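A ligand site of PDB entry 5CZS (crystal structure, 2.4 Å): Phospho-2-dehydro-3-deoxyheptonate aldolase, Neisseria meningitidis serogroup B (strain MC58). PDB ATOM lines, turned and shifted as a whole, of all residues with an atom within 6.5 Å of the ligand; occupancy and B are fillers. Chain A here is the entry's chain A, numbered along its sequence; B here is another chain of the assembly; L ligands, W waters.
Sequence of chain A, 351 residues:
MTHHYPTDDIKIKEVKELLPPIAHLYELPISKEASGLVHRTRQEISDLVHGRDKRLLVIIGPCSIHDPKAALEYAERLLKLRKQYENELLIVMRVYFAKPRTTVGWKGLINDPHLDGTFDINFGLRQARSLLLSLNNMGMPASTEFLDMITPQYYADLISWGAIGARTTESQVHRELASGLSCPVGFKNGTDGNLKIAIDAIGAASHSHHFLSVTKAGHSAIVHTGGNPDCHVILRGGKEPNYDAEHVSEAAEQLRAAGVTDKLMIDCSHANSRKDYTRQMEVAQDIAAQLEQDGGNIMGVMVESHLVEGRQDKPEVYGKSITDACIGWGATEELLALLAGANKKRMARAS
The backbone NH (N) of Ser 182 sits at hydrogen-bond distance from an oxygen (O1) of the ligand (2.9 Å). OG of Ser 182 sits at hydrogen-bond distance from O2 of the ligand, 2.6 Å away. An oxygen (O2) of the ligand sits at hydrogen-bond distance from the backbone NH (N) of Asp 9 of chain B (3.0 Å). OD1 of Asp 9 of chain B is in salt-bridge range of N1 of the ligand (2.7 Å). A nitrogen (N1) of the ligand sits at hydrogen-bond distance from the side-chain amide oxygen (OE1) of Gln 153 (2.9 Å). The side-chain carboxylate (OD1) of Asp 8 of chain B lies within salt-bridge range of a nitrogen (N1) of the ligand, at 3.4 Å.
Water W2 lies within hydrogen-bond range of a nitrogen (N1) of the ligand (2.6 Å), the side-chain carboxylate (OD1) of Asp 8 of chain B (2.7 Å) and the side-chain amino group (NZ) of Lys 216 (3.4 Å). Water W1 lies within hydrogen-bond range of O of Ala 156 (3.0 Å), O1 of the ligand (3.2 Å), NH2 of Arg 42 (3.3 Å) and SG of Cys 183 (3.3 Å).
Merely in contact with the ligand: Met 149, Pro 152, Ala 156, Leu 177, Gly 180, Leu 181, Phe 211, Ser 213, Lys 216 and Ile 12 of chain B. Hydrophobic or aromatic side chains that line the ligand: Pro 152, Ala 156, Leu 177, Leu 181, Phe 211 and Ile 12 of chain B. Of the 26 residues printed, 14 come within 4 Å of the ligand. The nearest printed residue that does not touch the ligand is Thr 7 of chain B (4.1 Å).
N of Asp 9 of chain B is in hydrogen-bond range of OG of Ser 182 (3.3 Å). The backbone carbonyl oxygen (O) of Ser 182 sits at hydrogen-bond distance from the side-chain amino group (NZ) of Lys 11 of chain B (3.1 Å). The side-chain amide oxygen (OE1) of Gln 153 sits at hydrogen-bond distance from the side-chain amino group (NZ) of Lys 216 (2.8 Å). The backbone carbonyl oxygen (O) of Val 214 sits at hydrogen-bond distance from the side-chain amide nitrogen (NE2) of Gln 153, at 2.7 Å. The side-chain amino group of Lys 216 lies within salt-bridge range of the side-chain carboxylate of Asp 8 of chain B (2.7 Å). OG of Ser 213 sits at hydrogen-bond distance from O of Met 149. The backbone carbonyl oxygen (O) of Phe 211 sits at hydrogen-bond distance from the backbone NH (N) of Val 223, 2.9 Å away. The side-chain amino group of Lys 11 of chain B lies within hydrogen-bond range of the backbone carbonyl oxygen of Leu 181 (3.0 Å).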
ATOM      1  N   ARG A  42     -15.220  23.743  -9.626  1.00  0.00           N
ATOM      2  CA  ARG A  42     -13.803  23.498  -9.941  1.00  0.00           C
ATOM      3  C   ARG A  42     -12.885  24.196  -8.934  1.00  0.00           C
ATOM      4  O   ARG A  42     -11.983  23.578  -8.399  1.00  0.00           O
ATOM      5  CB  ARG A  42     -13.446  23.962 -11.364  1.00  0.00           C
ATOM      6  CG  ARG A  42     -14.094  23.132 -12.463  1.00  0.00           C
ATOM      7  CD  ARG A  42     -13.959  23.761 -13.825  1.00  0.00           C
ATOM      8  NE  ARG A  42     -14.490  22.889 -14.864  1.00  0.00           N
ATOM      9  CZ  ARG A  42     -14.642  23.236 -16.153  1.00  0.00           C
ATOM     10  NH1 ARG A  42     -14.301  24.453 -16.549  1.00  0.00           N
ATOM     11  NH2 ARG A  42     -15.141  22.358 -17.031  1.00  0.00           N
ATOM     12  N   PHE A 146     -12.876  10.579 -18.629  1.00  0.00           N
ATOM     13  CA  PHE A 146     -12.613  10.733 -20.058  1.00  0.00           C
ATOM     14  C   PHE A 146     -11.725   9.579 -20.547  1.00  0.00           C
ATOM     15  O   PHE A 146     -10.582   9.440 -20.110  1.00  0.00           O
ATOM     16  CB  PHE A 146     -11.960  12.086 -20.334  1.00  0.00           C
ATOM     17  CG  PHE A 146     -12.848  13.251 -20.007  1.00  0.00           C
ATOM     18  CD1 PHE A 146     -13.945  13.557 -20.819  1.00  0.00           C
ATOM     19  CD2 PHE A 146     -12.597  14.053 -18.907  1.00  0.00           C
ATOM     20  CE1 PHE A 146     -14.754  14.639 -20.535  1.00  0.00           C
ATOM     21  CE2 PHE A 146     -13.402  15.135 -18.615  1.00  0.00           C
ATOM     22  CZ  PHE A 146     -14.472  15.436 -19.438  1.00  0.00           C
ATOM     23  N   MET A 149      -9.701  11.166 -26.236  1.00  0.00           N
ATOM     24  CA  MET A 149      -9.238  12.553 -26.348  1.00  0.00           C
ATOM     25  C   MET A 149     -10.173  13.402 -27.181  1.00  0.00           C
ATOM     26  O   MET A 149      -9.944  14.585 -27.359  1.00  0.00           O
ATOM     27  CB  MET A 149      -7.808  12.583 -26.971  1.00  0.00           C
ATOM     28  CG  MET A 149      -6.663  12.484 -25.962  1.00  0.00           C
ATOM     29  SD  MET A 149      -6.790  10.986 -24.972  1.00  0.00           S
ATOM     30  CE  MET A 149      -6.709   9.766 -26.276  1.00  0.00           C
ATOM     31  N   ILE A 150     -11.235  12.789 -27.697  1.00  0.00           N
ATOM     32  CA  ILE A 150     -12.222  13.535 -28.510  1.00  0.00           C
ATOM     33  C   ILE A 150     -13.494  13.906 -27.734  1.00  0.00           C
ATOM     34  O   ILE A 150     -13.925  15.050 -27.802  1.00  0.00           O
ATOM     35  CB  ILE A 150     -12.554  12.765 -29.792  1.00  0.00           C
ATOM     36  CG1 ILE A 150     -11.315  12.736 -30.672  1.00  0.00           C
ATOM     37  CG2 ILE A 150     -13.728  13.387 -30.538  1.00  0.00           C
ATOM     38  CD1 ILE A 150     -11.471  11.865 -31.887  1.00  0.00           C
ATOM     39  N   PRO A 152     -14.116  14.844 -24.672  1.00  0.00           N
ATOM     40  CA  PRO A 152     -14.156  16.101 -23.916  1.00  0.00           C
ATOM     41  C   PRO A 152     -14.713  17.349 -24.645  1.00  0.00           C
ATOM     42  O   PRO A 152     -15.232  18.260 -23.995  1.00  0.00           O
ATOM     43  CB  PRO A 152     -12.660  16.335 -23.559  1.00  0.00           C
ATOM     44  CG  PRO A 152     -12.039  14.998 -23.593  1.00  0.00           C
ATOM     45  CD  PRO A 152     -12.761  14.259 -24.692  1.00  0.00           C
ATOM     46  N   GLN A 153     -14.586  17.415 -25.974  1.00  0.00           N
ATOM     47  CA  GLN A 153     -14.976  18.621 -26.707  1.00  0.00           C
ATOM     48  C   GLN A 153     -16.477  18.745 -26.790  1.00  0.00           C
ATOM     49  O   GLN A 153     -17.003  19.823 -27.035  1.00  0.00           O
ATOM     50  CB  GLN A 153     -14.399  18.622 -28.114  1.00  0.00           C
ATOM     51  CG  GLN A 153     -12.884  18.732 -28.166  1.00  0.00           C
ATOM     52  CD  GLN A 153     -12.406  20.155 -27.938  1.00  0.00           C
ATOM     53  OE1 GLN A 153     -12.534  20.713 -26.844  1.00  0.00           O
ATOM     54  NE2 GLN A 153     -11.839  20.772 -28.992  1.00  0.00           N
ATOM     55  N   ALA A 156     -16.977  18.603 -21.866  1.00  0.00           N
ATOM     56  CA  ALA A 156     -16.072  18.814 -20.736  1.00  0.00           C
ATOM     57  C   ALA A 156     -16.385  20.124 -20.051  1.00  0.00           C
ATOM     58  O   ALA A 156     -16.177  20.259 -18.859  1.00  0.00           O
ATOM     59  CB  ALA A 156     -14.617  18.770 -21.164  1.00  0.00           C
ATOM     60  N   ASP A 157     -16.924  21.075 -20.810  1.00  0.00           N
ATOM     61  CA  ASP A 157     -17.320  22.358 -20.264  1.00  0.00           C
ATOM     62  C   ASP A 157     -18.345  22.260 -19.138  1.00  0.00           C
ATOM     63  O   ASP A 157     -18.492  23.218 -18.371  1.00  0.00           O
ATOM     64  CB  ASP A 157     -17.875  23.264 -21.363  1.00  0.00           C
ATOM     65  CG  ASP A 157     -19.065  22.668 -22.063  1.00  0.00           C
ATOM     66  OD1 ASP A 157     -19.039  21.460 -22.315  1.00  0.00           O
ATOM     67  OD2 ASP A 157     -20.015  23.394 -22.383  1.00  0.00           O
ATOM     68  N   LEU A 177      -3.802  14.724 -22.182  1.00  0.00           N
ATOM     69  CA  LEU A 177      -5.185  15.195 -22.107  1.00  0.00           C
ATOM     70  C   LEU A 177      -5.472  15.887 -20.785  1.00  0.00           C
ATOM     71  O   LEU A 177      -5.958  17.004 -20.765  1.00  0.00           O
ATOM     72  CB  LEU A 177      -6.162  14.014 -22.258  1.00  0.00           C
ATOM     73  CG  LEU A 177      -7.627  14.319 -21.869  1.00  0.00           C
ATOM     74  CD1 LEU A 177      -8.226  15.383 -22.765  1.00  0.00           C
ATOM     75  CD2 LEU A 177      -8.447  13.042 -21.923  1.00  0.00           C
ATOM     76  N   GLY A 180      -4.592  19.440 -20.143  1.00  0.00           N
ATOM     77  CA  GLY A 180      -5.457  20.462 -20.767  1.00  0.00           C
ATOM     78  C   GLY A 180      -6.935  20.446 -20.395  1.00  0.00           C
ATOM     79  O   GLY A 180      -7.726  21.187 -20.974  1.00  0.00           O
ATOM     80  N   LEU A 181      -7.331  19.608 -19.454  1.00  0.00           N
ATOM     81  CA  LEU A 181      -8.699  19.633 -18.965  1.00  0.00           C
ATOM     82  C   LEU A 181      -8.955  20.816 -18.044  1.00  0.00           C
ATOM     83  O   LEU A 181      -8.166  21.100 -17.168  1.00  0.00           O
ATOM     84  CB  LEU A 181      -9.032  18.322 -18.225  1.00  0.00           C
ATOM     85  CG  LEU A 181      -9.256  17.121 -19.164  1.00  0.00           C
ATOM     86  CD1 LEU A 181      -9.544  15.858 -18.356  1.00  0.00           C
ATOM     87  CD2 LEU A 181     -10.369  17.409 -20.164  1.00  0.00           C
ATOM     88  N   SER A 182     -10.082  21.491 -18.247  1.00  0.00           N
ATOM     89  CA  SER A 182     -10.461  22.652 -17.481  1.00  0.00           C
ATOM     90  C   SER A 182     -10.803  22.287 -16.032  1.00  0.00           C
ATOM     91  O   SER A 182     -10.713  23.119 -15.147  1.00  0.00           O
ATOM     92  CB  SER A 182     -11.667  23.342 -18.171  1.00  0.00           C
ATOM     93  OG  SER A 182     -11.363  23.757 -19.518  1.00  0.00           O
ATOM     94  N   CYS A 183     -11.156  21.034 -15.782  1.00  0.00           N
ATOM     95  CA  CYS A 183     -11.477  20.580 -14.460  1.00  0.00           C
ATOM     96  C   CYS A 183     -10.263  20.013 -13.719  1.00  0.00           C
ATOM     97  O   CYS A 183      -9.279  19.637 -14.343  1.00  0.00           O
ATOM     98  CB  CYS A 183     -12.528  19.503 -14.538  1.00  0.00           C
ATOM     99  SG  CYS A 183     -12.070  18.069 -15.510  1.00  0.00           S
ATOM    100  N   PHE A 211      -1.255  17.307 -27.771  1.00  0.00           N
ATOM    101  CA  PHE A 211      -1.868  16.042 -28.225  1.00  0.00           C
ATOM    102  C   PHE A 211      -2.821  16.281 -29.377  1.00  0.00           C
ATOM    103  O   PHE A 211      -3.195  17.427 -29.652  1.00  0.00           O
ATOM    104  CB  PHE A 211      -2.575  15.316 -27.101  1.00  0.00           C
ATOM    105  CG  PHE A 211      -3.777  16.039 -26.549  1.00  0.00           C
ATOM    106  CD1 PHE A 211      -3.626  16.991 -25.537  1.00  0.00           C
ATOM    107  CD2 PHE A 211      -5.056  15.742 -26.995  1.00  0.00           C
ATOM    108  CE1 PHE A 211      -4.722  17.639 -25.018  1.00  0.00           C
ATOM    109  CE2 PHE A 211      -6.161  16.391 -26.472  1.00  0.00           C
ATOM    110  CZ  PHE A 211      -6.001  17.359 -25.496  1.00  0.00           C
ATOM    111  N   LEU A 212      -3.215  15.207 -30.062  1.00  0.00           N
ATOM    112  CA  LEU A 212      -4.091  15.343 -31.225  1.00  0.00           C
ATOM    113  C   LEU A 212      -5.535  15.194 -30.802  1.00  0.00           C
ATOM    114  O   LEU A 212      -5.848  14.369 -29.983  1.00  0.00           O
ATOM    115  CB  LEU A 212      -3.747  14.352 -32.322  1.00  0.00           C
ATOM    116  CG  LEU A 212      -2.267  14.247 -32.696  1.00  0.00           C
ATOM    117  CD1 LEU A 212      -2.101  13.451 -33.979  1.00  0.00           C
ATOM    118  CD2 LEU A 212      -1.604  15.593 -32.890  1.00  0.00           C
ATOM    119  N   SER A 213      -6.428  16.022 -31.340  1.00  0.00           N
ATOM    120  CA  SER A 213      -7.859  15.850 -31.117  1.00  0.00           C
ATOM    121  C   SER A 213      -8.634  16.541 -32.244  1.00  0.00           C
ATOM    122  O   SER A 213      -8.138  16.579 -33.358  1.00  0.00           O
ATOM    123  CB  SER A 213      -8.273  16.371 -29.721  1.00  0.00           C
ATOM    124  OG  SER A 213      -9.697  16.277 -29.534  1.00  0.00           O
ATOM    125  N   VAL A 214      -9.835  17.049 -31.952  1.00  0.00           N
ATOM    126  CA  VAL A 214     -10.572  17.885 -32.911  1.00  0.00           C
ATOM    127  C   VAL A 214     -10.869  19.277 -32.352  1.00  0.00           C
ATOM    128  O   VAL A 214     -10.887  19.463 -31.143  1.00  0.00           O
ATOM    129  CB  VAL A 214     -11.882  17.225 -33.400  1.00  0.00           C
ATOM    130  CG1 VAL A 214     -11.563  15.981 -34.174  1.00  0.00           C
ATOM    131  CG2 VAL A 214     -12.802  16.873 -32.242  1.00  0.00           C
ATOM    132  N   LYS A 216     -13.644  22.517 -32.104  1.00  0.00           N
ATOM    133  CA  LYS A 216     -15.056  22.467 -31.824  1.00  0.00           C
ATOM    134  C   LYS A 216     -15.788  22.223 -33.134  1.00  0.00           C
ATOM    135  O   LYS A 216     -16.881  21.641 -33.128  1.00  0.00           O
ATOM    136  CB  LYS A 216     -15.547  23.768 -31.174  1.00  0.00           C
ATOM    137  CG  LYS A 216     -15.095  23.955 -29.726  1.00  0.00           C
ATOM    138  CD  LYS A 216     -15.434  22.752 -28.854  1.00  0.00           C
ATOM    139  CE  LYS A 216     -15.385  23.096 -27.358  1.00  0.00           C
ATOM    140  NZ  LYS A 216     -13.997  23.132 -26.817  1.00  0.00           N
ATOM    141  N   VAL A 223      -3.486  20.230 -30.108  1.00  0.00           N
ATOM    142  CA  VAL A 223      -3.831  21.073 -28.957  1.00  0.00           C
ATOM    143  C   VAL A 223      -2.689  21.245 -27.978  1.00  0.00           C
ATOM    144  O   VAL A 223      -2.106  20.263 -27.497  1.00  0.00           O
ATOM    145  CB  VAL A 223      -5.157  20.681 -28.237  1.00  0.00           C
ATOM    146  CG1 VAL A 223      -5.885  19.539 -28.935  1.00  0.00           C
ATOM    147  CG2 VAL A 223      -4.968  20.419 -26.758  1.00  0.00           C
ATOM    148  N   THR B   7     -16.011  28.326 -18.904  1.00  0.00           N
ATOM    149  CA  THR B   7     -15.786  26.935 -18.450  1.00  0.00           C
ATOM    150  C   THR B   7     -15.106  26.054 -19.490  1.00  0.00           C
ATOM    151  O   THR B   7     -14.825  24.889 -19.221  1.00  0.00           O
ATOM    152  CB  THR B   7     -17.104  26.243 -18.048  1.00  0.00           C
ATOM    153  OG1 THR B   7     -17.971  26.147 -19.183  1.00  0.00           O
ATOM    154  CG2 THR B   7     -17.792  27.005 -16.982  1.00  0.00           C
ATOM    155  N   ASP B   8     -14.819  26.611 -20.668  1.00  0.00           N
ATOM    156  CA  ASP B   8     -14.324  25.879 -21.816  1.00  0.00           C
ATOM    157  C   ASP B   8     -12.941  26.326 -22.126  1.00  0.00           C
ATOM    158  O   ASP B   8     -12.703  27.522 -22.210  1.00  0.00           O
ATOM    159  CB  ASP B   8     -15.220  26.177 -23.035  1.00  0.00           C
ATOM    160  CG  ASP B   8     -14.659  25.620 -24.351  1.00  0.00           C
ATOM    161  OD1 ASP B   8     -14.218  24.436 -24.428  1.00  0.00           O
ATOM    162  OD2 ASP B   8     -14.680  26.391 -25.324  1.00  0.00           O
ATOM    163  N   ASP B   9     -12.045  25.368 -22.326  1.00  0.00           N
ATOM    164  CA  ASP B   9     -10.629  25.604 -22.716  1.00  0.00           C
ATOM    165  C   ASP B   9      -9.837  26.480 -21.709  1.00  0.00           C
ATOM    166  O   ASP B   9      -8.921  27.188 -22.086  1.00  0.00           O
ATOM    167  CB  ASP B   9     -10.553  26.175 -24.173  1.00  0.00           C
ATOM    168  CG  ASP B   9     -10.733  25.092 -25.260  1.00  0.00           C
ATOM    169  OD1 ASP B   9     -10.995  23.910 -24.950  1.00  0.00           O
ATOM    170  OD2 ASP B   9     -10.618  25.448 -26.464  1.00  0.00           O
ATOM    171  N   ILE B  10     -10.176  26.390 -20.434  1.00  0.00           N
ATOM    172  CA  ILE B  10      -9.513  27.194 -19.396  1.00  0.00           C
ATOM    173  C   ILE B  10      -8.000  27.033 -19.405  1.00  0.00           C
ATOM    174  O   ILE B  10      -7.257  28.020 -19.298  1.00  0.00           O
ATOM    175  CB  ILE B  10     -10.019  26.851 -17.954  1.00  0.00           C
ATOM    176  CG1 ILE B  10     -11.530  27.088 -17.838  1.00  0.00           C
ATOM    177  CG2 ILE B  10      -9.301  27.679 -16.896  1.00  0.00           C
ATOM    178  CD1 ILE B  10     -11.952  28.453 -18.309  1.00  0.00           C
ATOM    179  N   LYS B  11      -7.560  25.794 -19.569  1.00  0.00           N
ATOM    180  CA  LYS B  11      -6.143  25.480 -19.462  1.00  0.00           C
ATOM    181  C   LYS B  11      -5.545  25.129 -20.792  1.00  0.00           C
ATOM    182  O   LYS B  11      -4.613  24.325 -20.855  1.00  0.00           O
ATOM    183  CB  LYS B  11      -5.944  24.343 -18.477  1.00  0.00           C
ATOM    184  CG  LYS B  11      -6.524  24.643 -17.111  1.00  0.00           C
ATOM    185  CD  LYS B  11      -6.312  23.493 -16.142  1.00  0.00           C
ATOM    186  CE  LYS B  11      -7.251  23.639 -14.953  1.00  0.00           C
ATOM    187  NZ  LYS B  11      -7.765  22.340 -14.441  1.00  0.00           N
ATOM    188  N   ILE B  12      -6.059  25.738 -21.866  1.00  0.00           N
ATOM    189  CA  ILE B  12      -5.609  25.486 -23.221  1.00  0.00           C
ATOM    190  C   ILE B  12      -4.912  26.730 -23.744  1.00  0.00           C
ATOM    191  O   ILE B  12      -5.511  27.789 -23.763  1.00  0.00           O
ATOM    192  CB  ILE B  12      -6.793  25.191 -24.150  1.00  0.00           C
ATOM    193  CG1 ILE B  12      -7.503  23.893 -23.742  1.00  0.00           C
ATOM    194  CG2 ILE B  12      -6.346  25.148 -25.590  1.00  0.00           C
ATOM    195  CD1 ILE B  12      -6.647  22.649 -23.720  1.00  0.00           C
ATOM    196  N   VAL B  15      -5.554  25.725 -29.757  1.00  0.00           N
ATOM    197  CA  VAL B  15      -5.962  24.577 -30.554  1.00  0.00           C
ATOM    198  C   VAL B  15      -5.844  24.990 -32.009  1.00  0.00           C
ATOM    199  O   VAL B  15      -6.641  25.800 -32.467  1.00  0.00           O
ATOM    200  CB  VAL B  15      -7.421  24.129 -30.267  1.00  0.00           C
ATOM    201  CG1 VAL B  15      -7.817  22.972 -31.189  1.00  0.00           C
ATOM    202  CG2 VAL B  15      -7.597  23.733 -28.800  1.00  0.00           C
HETATM  203  N1  LIG L   1     -12.214  21.682 -24.107  1.00  0.00           N
HETATM  204  C1  LIG L   1     -11.583  20.855 -23.039  1.00  0.00           C
HETATM  205  C2  LIG L   1     -11.895  21.453 -21.664  1.00  0.00           C
HETATM  206  O1  LIG L   1     -11.627  20.804 -20.641  1.00  0.00           O
HETATM  207  C3  LIG L   1     -10.071  20.692 -23.285  1.00  0.00           C
HETATM  208  C4  LIG L   1      -9.768  19.950 -24.549  1.00  0.00           C
HETATM  209  C5  LIG L   1      -9.667  20.622 -25.746  1.00  0.00           C
HETATM  210  C6  LIG L   1      -9.688  18.565 -24.553  1.00  0.00           C
HETATM  211  C7  LIG L   1      -9.468  19.927 -26.934  1.00  0.00           C
HETATM  212  C8  LIG L   1      -9.490  17.861 -25.741  1.00  0.00           C
HETATM  213  C9  LIG L   1      -9.385  18.543 -26.929  1.00  0.00           C
HETATM  214  O2  LIG L   1     -12.468  22.545 -21.554  1.00  0.00           O
HETATM  215  O   HOH W   1     -13.317  19.776 -18.106  1.00  0.00           O
HETATM  216  O   HOH W   2     -14.736  21.908 -23.681  1.00  0.00           O
